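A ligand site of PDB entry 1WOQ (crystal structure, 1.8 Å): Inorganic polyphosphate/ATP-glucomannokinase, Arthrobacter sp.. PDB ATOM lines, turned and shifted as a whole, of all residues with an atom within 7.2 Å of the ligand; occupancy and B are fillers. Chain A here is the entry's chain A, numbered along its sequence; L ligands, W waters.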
ATOM      1  N   ILE A  19      20.631 -15.091  19.530  1.00  0.00           N
ATOM      2  CA  ILE A  19      20.827 -14.868  18.101  1.00  0.00           C
ATOM      3  C   ILE A  19      21.852 -13.752  17.888  1.00  0.00           C
ATOM      4  O   ILE A  19      21.598 -12.593  18.214  1.00  0.00           O
ATOM      5  CB  ILE A  19      19.510 -14.483  17.402  1.00  0.00           C
ATOM      6  CG1 ILE A  19      18.499 -15.625  17.526  1.00  0.00           C
ATOM      7  CG2 ILE A  19      19.769 -14.151  15.934  1.00  0.00           C
ATOM      8  CD1 ILE A  19      17.117 -15.308  16.999  1.00  0.00           C
ATOM      9  N   GLY A  20      23.013 -14.123  17.355  1.00  0.00           N
ATOM     10  CA  GLY A  20      24.050 -13.146  17.125  1.00  0.00           C
ATOM     11  C   GLY A  20      24.337 -12.914  15.656  1.00  0.00           C
ATOM     12  O   GLY A  20      23.731 -13.553  14.793  1.00  0.00           O
ATOM     13  N   GLY A  21      25.274 -12.012  15.369  1.00  0.00           N
ATOM     14  CA  GLY A  21      25.614 -11.713  13.998  1.00  0.00           C
ATOM     15  C   GLY A  21      26.336 -12.857  13.300  1.00  0.00           C
ATOM     16  O   GLY A  21      26.106 -13.094  12.113  1.00  0.00           O
ATOM     17  N   PHE A  82      17.251 -11.226  20.412  1.00  0.00           N
ATOM     18  CA  PHE A  82      17.273 -10.675  19.067  1.00  0.00           C
ATOM     19  C   PHE A  82      17.873  -9.280  19.159  1.00  0.00           C
ATOM     20  O   PHE A  82      17.523  -8.513  20.050  1.00  0.00           O
ATOM     21  CB  PHE A  82      15.856 -10.584  18.494  1.00  0.00           C
ATOM     22  CG  PHE A  82      15.825 -10.143  17.067  1.00  0.00           C
ATOM     23  CD1 PHE A  82      15.977 -11.065  16.039  1.00  0.00           C
ATOM     24  CD2 PHE A  82      15.696  -8.792  16.754  1.00  0.00           C
ATOM     25  CE1 PHE A  82      16.014 -10.648  14.714  1.00  0.00           C
ATOM     26  CE2 PHE A  82      15.733  -8.365  15.430  1.00  0.00           C
ATOM     27  CZ  PHE A  82      15.894  -9.298  14.406  1.00  0.00           C
ATOM     28  N   PRO A  83      18.775  -8.927  18.229  1.00  0.00           N
ATOM     29  CA  PRO A  83      19.420  -7.619  18.228  1.00  0.00           C
ATOM     30  C   PRO A  83      18.558  -6.460  17.749  1.00  0.00           C
ATOM     31  O   PRO A  83      18.894  -5.805  16.760  1.00  0.00           O
ATOM     32  CB  PRO A  83      20.645  -7.844  17.349  1.00  0.00           C
ATOM     33  CG  PRO A  83      20.099  -8.747  16.303  1.00  0.00           C
ATOM     34  CD  PRO A  83      19.275  -9.746  17.100  1.00  0.00           C
ATOM     35  N   GLY A  84      17.458  -6.184  18.451  1.00  0.00           N
ATOM     36  CA  GLY A  84      16.596  -5.080  18.068  1.00  0.00           C
ATOM     37  C   GLY A  84      15.534  -4.817  19.114  1.00  0.00           C
ATOM     38  O   GLY A  84      15.423  -5.547  20.101  1.00  0.00           O
ATOM     39  N   ILE A  85      14.755  -3.758  18.908  1.00  0.00           N
ATOM     40  CA  ILE A  85      13.675  -3.415  19.830  1.00  0.00           C
ATOM     41  C   ILE A  85      12.593  -4.492  19.716  1.00  0.00           C
ATOM     42  O   ILE A  85      12.155  -4.826  18.604  1.00  0.00           O
ATOM     43  CB  ILE A  85      13.043  -2.055  19.455  1.00  0.00           C
ATOM     44  CG1 ILE A  85      14.079  -0.943  19.595  1.00  0.00           C
ATOM     45  CG2 ILE A  85      11.843  -1.772  20.358  1.00  0.00           C
ATOM     46  CD1 ILE A  85      13.621   0.410  19.028  1.00  0.00           C
ATOM     47  N   SER A  93      13.155  -2.815  15.199  1.00  0.00           N
ATOM     48  CA  SER A  93      14.406  -2.248  14.697  1.00  0.00           C
ATOM     49  C   SER A  93      15.259  -3.409  14.196  1.00  0.00           C
ATOM     50  O   SER A  93      15.156  -4.522  14.709  1.00  0.00           O
ATOM     51  CB  SER A  93      15.153  -1.449  15.781  1.00  0.00           C
ATOM     52  OG  SER A  93      15.710  -2.297  16.766  1.00  0.00           O
ATOM     53  N   ALA A  94      16.093  -3.137  13.192  1.00  0.00           N
ATOM     54  CA  ALA A  94      16.956  -4.176  12.625  1.00  0.00           C
ATOM     55  C   ALA A  94      18.223  -3.508  12.126  1.00  0.00           C
ATOM     56  O   ALA A  94      18.568  -3.603  10.948  1.00  0.00           O
ATOM     57  CB  ALA A  94      16.233  -4.873  11.467  1.00  0.00           C
ATOM     58  N   ALA A  95      18.912  -2.823  13.031  1.00  0.00           N
ATOM     59  CA  ALA A  95      20.127  -2.100  12.697  1.00  0.00           C
ATOM     60  C   ALA A  95      21.157  -2.901  11.916  1.00  0.00           C
ATOM     61  O   ALA A  95      21.689  -2.421  10.903  1.00  0.00           O
ATOM     62  CB  ALA A  95      20.756  -1.544  13.965  1.00  0.00           C
ATOM     63  N   ASN A  96      21.457  -4.108  12.372  1.00  0.00           N
ATOM     64  CA  ASN A  96      22.482  -4.906  11.704  1.00  0.00           C
ATOM     65  C   ASN A  96      22.024  -6.280  11.232  1.00  0.00           C
ATOM     66  O   ASN A  96      22.809  -7.226  11.169  1.00  0.00           O
ATOM     67  CB  ASN A  96      23.686  -5.036  12.637  1.00  0.00           C
ATOM     68  CG  ASN A  96      24.199  -3.679  13.091  1.00  0.00           C
ATOM     69  OD1 ASN A  96      24.181  -3.356  14.281  1.00  0.00           O
ATOM     70  ND2 ASN A  96      24.652  -2.875  12.134  1.00  0.00           N
ATOM     71  N   ASN A 122      15.279  -8.380  23.702  1.00  0.00           N
ATOM     72  CA  ASN A 122      16.463  -7.788  23.097  1.00  0.00           C
ATOM     73  C   ASN A 122      17.722  -8.447  23.661  1.00  0.00           C
ATOM     74  O   ASN A 122      17.793  -8.749  24.845  1.00  0.00           O
ATOM     75  CB  ASN A 122      16.499  -6.289  23.353  1.00  0.00           C
ATOM     76  CG  ASN A 122      17.812  -5.665  22.953  1.00  0.00           C
ATOM     77  OD1 ASN A 122      18.689  -5.473  23.791  1.00  0.00           O
ATOM     78  ND2 ASN A 122      17.955  -5.364  21.670  1.00  0.00           N
ATOM     79  N   ASP A 123      18.726  -8.661  22.811  1.00  0.00           N
ATOM     80  CA  ASP A 123      19.955  -9.310  23.243  1.00  0.00           C
ATOM     81  C   ASP A 123      20.705  -8.598  24.373  1.00  0.00           C
ATOM     82  O   ASP A 123      21.191  -9.248  25.304  1.00  0.00           O
ATOM     83  CB  ASP A 123      20.898  -9.542  22.043  1.00  0.00           C
ATOM     84  CG  ASP A 123      21.354  -8.248  21.389  1.00  0.00           C
ATOM     85  OD1 ASP A 123      22.473  -8.259  20.810  1.00  0.00           O
ATOM     86  OD2 ASP A 123      20.623  -7.236  21.423  1.00  0.00           O
ATOM     87  N   ALA A 124      20.807  -7.270  24.302  1.00  0.00           N
ATOM     88  CA  ALA A 124      21.494  -6.516  25.345  1.00  0.00           C
ATOM     89  C   ALA A 124      20.675  -6.569  26.637  1.00  0.00           C
ATOM     90  O   ALA A 124      21.240  -6.686  27.735  1.00  0.00           O
ATOM     91  CB  ALA A 124      21.728  -5.067  24.904  1.00  0.00           C
ATOM     92  N   ASP A 125      19.354  -6.485  26.512  1.00  0.00           N
ATOM     93  CA  ASP A 125      18.461  -6.548  27.668  1.00  0.00           C
ATOM     94  C   ASP A 125      18.669  -7.871  28.401  1.00  0.00           C
ATOM     95  O   ASP A 125      18.695  -7.919  29.636  1.00  0.00           O
ATOM     96  CB  ASP A 125      16.997  -6.422  27.249  1.00  0.00           C
ATOM     97  CG  ASP A 125      16.585  -4.996  26.940  1.00  0.00           C
ATOM     98  OD1 ASP A 125      17.428  -4.083  27.031  1.00  0.00           O
ATOM     99  OD2 ASP A 125      15.397  -4.787  26.608  1.00  0.00           O
ATOM    100  N   THR A 148      27.143  -3.327  25.741  1.00  0.00           N
ATOM    101  CA  THR A 148      27.819  -4.412  25.050  1.00  0.00           C
ATOM    102  C   THR A 148      28.506  -3.920  23.779  1.00  0.00           C
ATOM    103  O   THR A 148      27.927  -3.162  22.988  1.00  0.00           O
ATOM    104  CB  THR A 148      26.829  -5.552  24.700  1.00  0.00           C
ATOM    105  OG1 THR A 148      25.853  -5.084  23.766  1.00  0.00           O
ATOM    106  CG2 THR A 148      26.121  -6.041  25.948  1.00  0.00           C
ATOM    107  N   LEU A 149      29.760  -4.342  23.591  1.00  0.00           N
ATOM    108  CA  LEU A 149      30.541  -3.935  22.428  1.00  0.00           C
ATOM    109  C   LEU A 149      30.769  -5.124  21.503  1.00  0.00           C
ATOM    110  O   LEU A 149      31.445  -6.087  21.863  1.00  0.00           O
ATOM    111  CB  LEU A 149      31.879  -3.362  22.892  1.00  0.00           C
ATOM    112  CG  LEU A 149      31.801  -2.213  23.895  1.00  0.00           C
ATOM    113  CD1 LEU A 149      33.193  -1.867  24.398  1.00  0.00           C
ATOM    114  CD2 LEU A 149      31.157  -1.001  23.234  1.00  0.00           C
ATOM    115  N   GLY A 150      30.200  -5.062  20.301  1.00  0.00           N
ATOM    116  CA  GLY A 150      30.364  -6.158  19.355  1.00  0.00           C
ATOM    117  C   GLY A 150      30.044  -5.657  17.961  1.00  0.00           C
ATOM    118  O   GLY A 150      30.542  -4.613  17.554  1.00  0.00           O
ATOM    119  N   THR A 151      29.218  -6.401  17.235  1.00  0.00           N
ATOM    120  CA  THR A 151      28.827  -5.998  15.876  1.00  0.00           C
ATOM    121  C   THR A 151      28.194  -4.614  16.004  1.00  0.00           C
ATOM    122  O   THR A 151      28.464  -3.710  15.227  1.00  0.00           O
ATOM    123  CB  THR A 151      27.823  -6.998  15.275  1.00  0.00           C
ATOM    124  OG1 THR A 151      28.456  -8.267  15.120  1.00  0.00           O
ATOM    125  CG2 THR A 151      27.337  -6.515  13.911  1.00  0.00           C
ATOM    126  N   GLY A 152      27.341  -4.471  17.008  1.00  0.00           N
ATOM    127  CA  GLY A 152      26.704  -3.186  17.256  1.00  0.00           C
ATOM    128  C   GLY A 152      26.988  -2.857  18.710  1.00  0.00           C
ATOM    129  O   GLY A 152      27.742  -3.562  19.376  1.00  0.00           O
ATOM    130  N   ILE A 153      26.419  -1.761  19.208  1.00  0.00           N
ATOM    131  CA  ILE A 153      26.584  -1.417  20.609  1.00  0.00           C
ATOM    132  C   ILE A 153      25.220  -1.621  21.234  1.00  0.00           C
ATOM    133  O   ILE A 153      24.241  -1.010  20.820  1.00  0.00           O
ATOM    134  CB  ILE A 153      27.040   0.040  20.804  1.00  0.00           C
ATOM    135  CG1 ILE A 153      28.484   0.197  20.297  1.00  0.00           C
ATOM    136  CG2 ILE A 153      26.945   0.427  22.286  1.00  0.00           C
ATOM    137  CD1 ILE A 153      29.071   1.595  20.497  1.00  0.00           C
ATOM    138  N   GLY A 154      25.155  -2.503  22.223  1.00  0.00           N
ATOM    139  CA  GLY A 154      23.893  -2.761  22.885  1.00  0.00           C
ATOM    140  C   GLY A 154      23.881  -2.120  24.247  1.00  0.00           C
ATOM    141  O   GLY A 154      24.936  -1.767  24.782  1.00  0.00           O
ATOM    142  N   SER A 155      22.699  -1.958  24.815  1.00  0.00           N
ATOM    143  CA  SER A 155      22.591  -1.374  26.137  1.00  0.00           C
ATOM    144  C   SER A 155      21.396  -1.919  26.893  1.00  0.00           C
ATOM    145  O   SER A 155      20.283  -1.959  26.354  1.00  0.00           O
ATOM    146  CB  SER A 155      22.472   0.154  26.055  1.00  0.00           C
ATOM    147  OG  SER A 155      21.270   0.525  25.395  1.00  0.00           O
ATOM    148  N   ASN A 166      14.297  -2.197  26.336  1.00  0.00           N
ATOM    149  CA  ASN A 166      14.603  -1.597  25.042  1.00  0.00           C
ATOM    150  C   ASN A 166      15.395  -0.294  24.961  1.00  0.00           C
ATOM    151  O   ASN A 166      15.139   0.506  24.068  1.00  0.00           O
ATOM    152  CB  ASN A 166      13.293  -1.462  24.259  1.00  0.00           C
ATOM    153  CG  ASN A 166      12.672  -2.809  23.920  1.00  0.00           C
ATOM    154  OD1 ASN A 166      11.490  -3.056  24.189  1.00  0.00           O
ATOM    155  ND2 ASN A 166      13.472  -3.693  23.320  1.00  0.00           N
ATOM    156  N   ALA A 167      16.341  -0.080  25.863  1.00  0.00           N
ATOM    157  CA  ALA A 167      17.145   1.147  25.752  1.00  0.00           C
ATOM    158  C   ALA A 167      18.084   0.894  24.558  1.00  0.00           C
ATOM    159  O   ALA A 167      18.736  -0.156  24.496  1.00  0.00           O
ATOM    160  CB  ALA A 167      17.958   1.383  27.024  1.00  0.00           C
ATOM    161  N   GLU A 168      18.146   1.838  23.624  1.00  0.00           N
ATOM    162  CA  GLU A 168      19.002   1.682  22.446  1.00  0.00           C
ATOM    163  C   GLU A 168      20.118   2.718  22.432  1.00  0.00           C
ATOM    164  O   GLU A 168      20.272   3.466  21.472  1.00  0.00           O
ATOM    165  CB  GLU A 168      18.163   1.802  21.160  1.00  0.00           C
ATOM    166  CG  GLU A 168      17.307   0.569  20.846  1.00  0.00           C
ATOM    167  CD  GLU A 168      18.128  -0.602  20.338  1.00  0.00           C
ATOM    168  OE1 GLU A 168      19.175  -0.360  19.692  1.00  0.00           O
ATOM    169  OE2 GLU A 168      17.726  -1.767  20.558  1.00  0.00           O
ATOM    170  N   GLY A 170      23.114   2.415  21.898  1.00  0.00           N
ATOM    171  CA  GLY A 170      24.129   2.206  20.882  1.00  0.00           C
ATOM    172  C   GLY A 170      23.826   3.109  19.712  1.00  0.00           C
ATOM    173  O   GLY A 170      24.648   3.275  18.800  1.00  0.00           O
ATOM    174  N   HIS A 171      22.635   3.721  19.724  1.00  0.00           N
ATOM    175  CA  HIS A 171      22.225   4.597  18.642  1.00  0.00           C
ATOM    176  C   HIS A 171      22.127   6.066  19.014  1.00  0.00           C
ATOM    177  O   HIS A 171      21.485   6.858  18.320  1.00  0.00           O
ATOM    178  CB  HIS A 171      20.935   4.071  18.015  1.00  0.00           C
ATOM    179  CG  HIS A 171      21.118   2.754  17.322  1.00  0.00           C
ATOM    180  ND1 HIS A 171      21.978   2.590  16.260  1.00  0.00           N
ATOM    181  CD2 HIS A 171      20.637   1.516  17.612  1.00  0.00           C
ATOM    182  CE1 HIS A 171      22.028   1.319  15.916  1.00  0.00           C
ATOM    183  NE2 HIS A 171      21.230   0.642  16.724  1.00  0.00           N
ATOM    184  N   ASP A 178      26.160   8.040  14.397  1.00  0.00           N
ATOM    185  CA  ASP A 178      25.438   7.062  15.198  1.00  0.00           C
ATOM    186  C   ASP A 178      26.583   6.447  15.994  1.00  0.00           C
ATOM    187  O   ASP A 178      27.573   5.999  15.411  1.00  0.00           O
ATOM    188  CB  ASP A 178      24.767   6.046  14.283  1.00  0.00           C
ATOM    189  CG  ASP A 178      24.225   4.859  15.022  1.00  0.00           C
ATOM    190  OD1 ASP A 178      25.022   3.960  15.380  1.00  0.00           O
ATOM    191  OD2 ASP A 178      23.001   4.818  15.267  1.00  0.00           O
ATOM    192  N   GLU A 180      27.421   3.594  17.479  1.00  0.00           N
ATOM    193  CA  GLU A 180      28.018   2.316  17.117  1.00  0.00           C
ATOM    194  C   GLU A 180      28.715   2.284  15.765  1.00  0.00           C
ATOM    195  O   GLU A 180      29.543   1.396  15.527  1.00  0.00           O
ATOM    196  CB  GLU A 180      26.982   1.182  17.182  1.00  0.00           C
ATOM    197  CG  GLU A 180      25.858   1.263  16.181  1.00  0.00           C
ATOM    198  CD  GLU A 180      25.059  -0.027  16.111  1.00  0.00           C
ATOM    199  OE1 GLU A 180      24.762  -0.593  17.184  1.00  0.00           O
ATOM    200  OE2 GLU A 180      24.721  -0.469  14.991  1.00  0.00           O
HETATM  201  C1  LIG L   1      20.873  -2.883  18.016  1.00  0.00           C
HETATM  202  C2  LIG L   1      20.519  -3.310  19.439  1.00  0.00           C
HETATM  203  C3  LIG L   1      21.431  -4.464  19.889  1.00  0.00           C
HETATM  204  C4  LIG L   1      22.898  -4.062  19.701  1.00  0.00           C
HETATM  205  C5  LIG L   1      23.887  -5.167  20.040  1.00  0.00           C
HETATM  206  C6  LIG L   1      22.362  -2.539  17.948  1.00  0.00           C
HETATM  207  O1  LIG L   1      22.729  -2.182  16.660  1.00  0.00           O
HETATM  208  O2  LIG L   1      20.092  -1.757  17.636  1.00  0.00           O
HETATM  209  O3  LIG L   1      19.160  -3.723  19.511  1.00  0.00           O
HETATM  210  O4  LIG L   1      21.186  -4.780  21.252  1.00  0.00           O
HETATM  211  O5  LIG L   1      23.143  -3.674  18.327  1.00  0.00           O
HETATM  212  O6  LIG L   1      23.585  -6.359  19.326  1.00  0.00           O
HETATM  213  O   HOH W   1      18.328  -3.058  15.932  1.00  0.00           O
HETATM  214  O   HOH W   2      23.294  -5.560  16.131  1.00  0.00           O
HETATM  215  O   HOH W   3      20.525  -2.580  22.854  1.00  0.00           O
HETATM  216  O   HOH W   4      26.215  -6.794  18.612  1.00  0.00           O
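OD2 of Asp 123 lies within hydrogen-bond range of O4 of the ligand (2.5 Å). The side-chain carboxylate (OE1) of Glu 180 sits at hydrogen-bond distance from an oxygen (O1) of the ligand. OE2 of Glu 168 is in hydrogen-bond range of O3 of the ligand (2.6 Å). NE2 of His 171 lies within hydrogen-bond range of O2 of the ligand, at 2.8 Å. The side-chain amide nitrogen (ND2) of Asn 122 is in hydrogen-bond range of an oxygen (O3) of the ligand (3.0 Å). The side-chain amide oxygen (OD1) of Asn 96 lies within hydrogen-bond range of an oxygen (O1) of the ligand. The backbone NH (N) of Gly 84 sits at hydrogen-bond distance from an oxygen (O3) of the ligand, 3.2 Å away. O of Pro 83 sits close to O3 of the ligand (3.5 Å).
Residues that only touch the ligand: Ala 95, Ile 153, Gly 154, Ala 124 and Gly 152. Of the 30 residues printed, 13 come within 4 Å of the ligand.
Water W4 lies within hydrogen-bond range of O6 of the ligand (2.8 Å), N of Gly 152 (3.0 Å) and N of Thr 151 (3.3 Å). Water W1 lies within hydrogen-bond range of an oxygen (O2) of the ligand (2.8 Å), the side-chain hydroxyl of Ser 93 (2.9 Å), the backbone carbonyl oxygen of Pro 83 (2.9 Å) and the backbone NH of Ala 95 (3.0 Å). Water W3 lies within hydrogen-bond range of O4 of the ligand (2.8 Å), N of Ser 155 (3.0 Å) and O of Ala 167 (3.4 Å). Water W2 lies within hydrogen-bond range of an oxygen (O5) of the ligand (2.9 Å) and the side-chain amide oxygen of Asn 96 (3.0 Å).
OD2 of Asp 123 lies within hydrogen-bond range of ND2 of Asn 122, at 3.3 Å. O of Phe 82 sits at hydrogen-bond distance from N of Asp 123, at 3.0 Å. The side-chain carboxylate of Glu 180 lies close to the side-chain amide oxygen of Asn 96, 3.0 Å away. The backbone NH of Ile 153 sits at hydrogen-bond distance from the side-chain carboxylate of Glu 180 (2.9 Å). N of Glu 180 sits close to OD1 of Asp 178 (3.2 Å). O of Gly 84 sits at hydrogen-bond distance from ND2 of Asn 122 (3.0 Å). N of Ala 124 lies within hydrogen-bond range of OD1 of Asn 122 (2.8 Å). The backbone carbonyl oxygen of Gly 154 is in hydrogen-bond range of the backbone NH of Thr 148 (2.9 Å).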
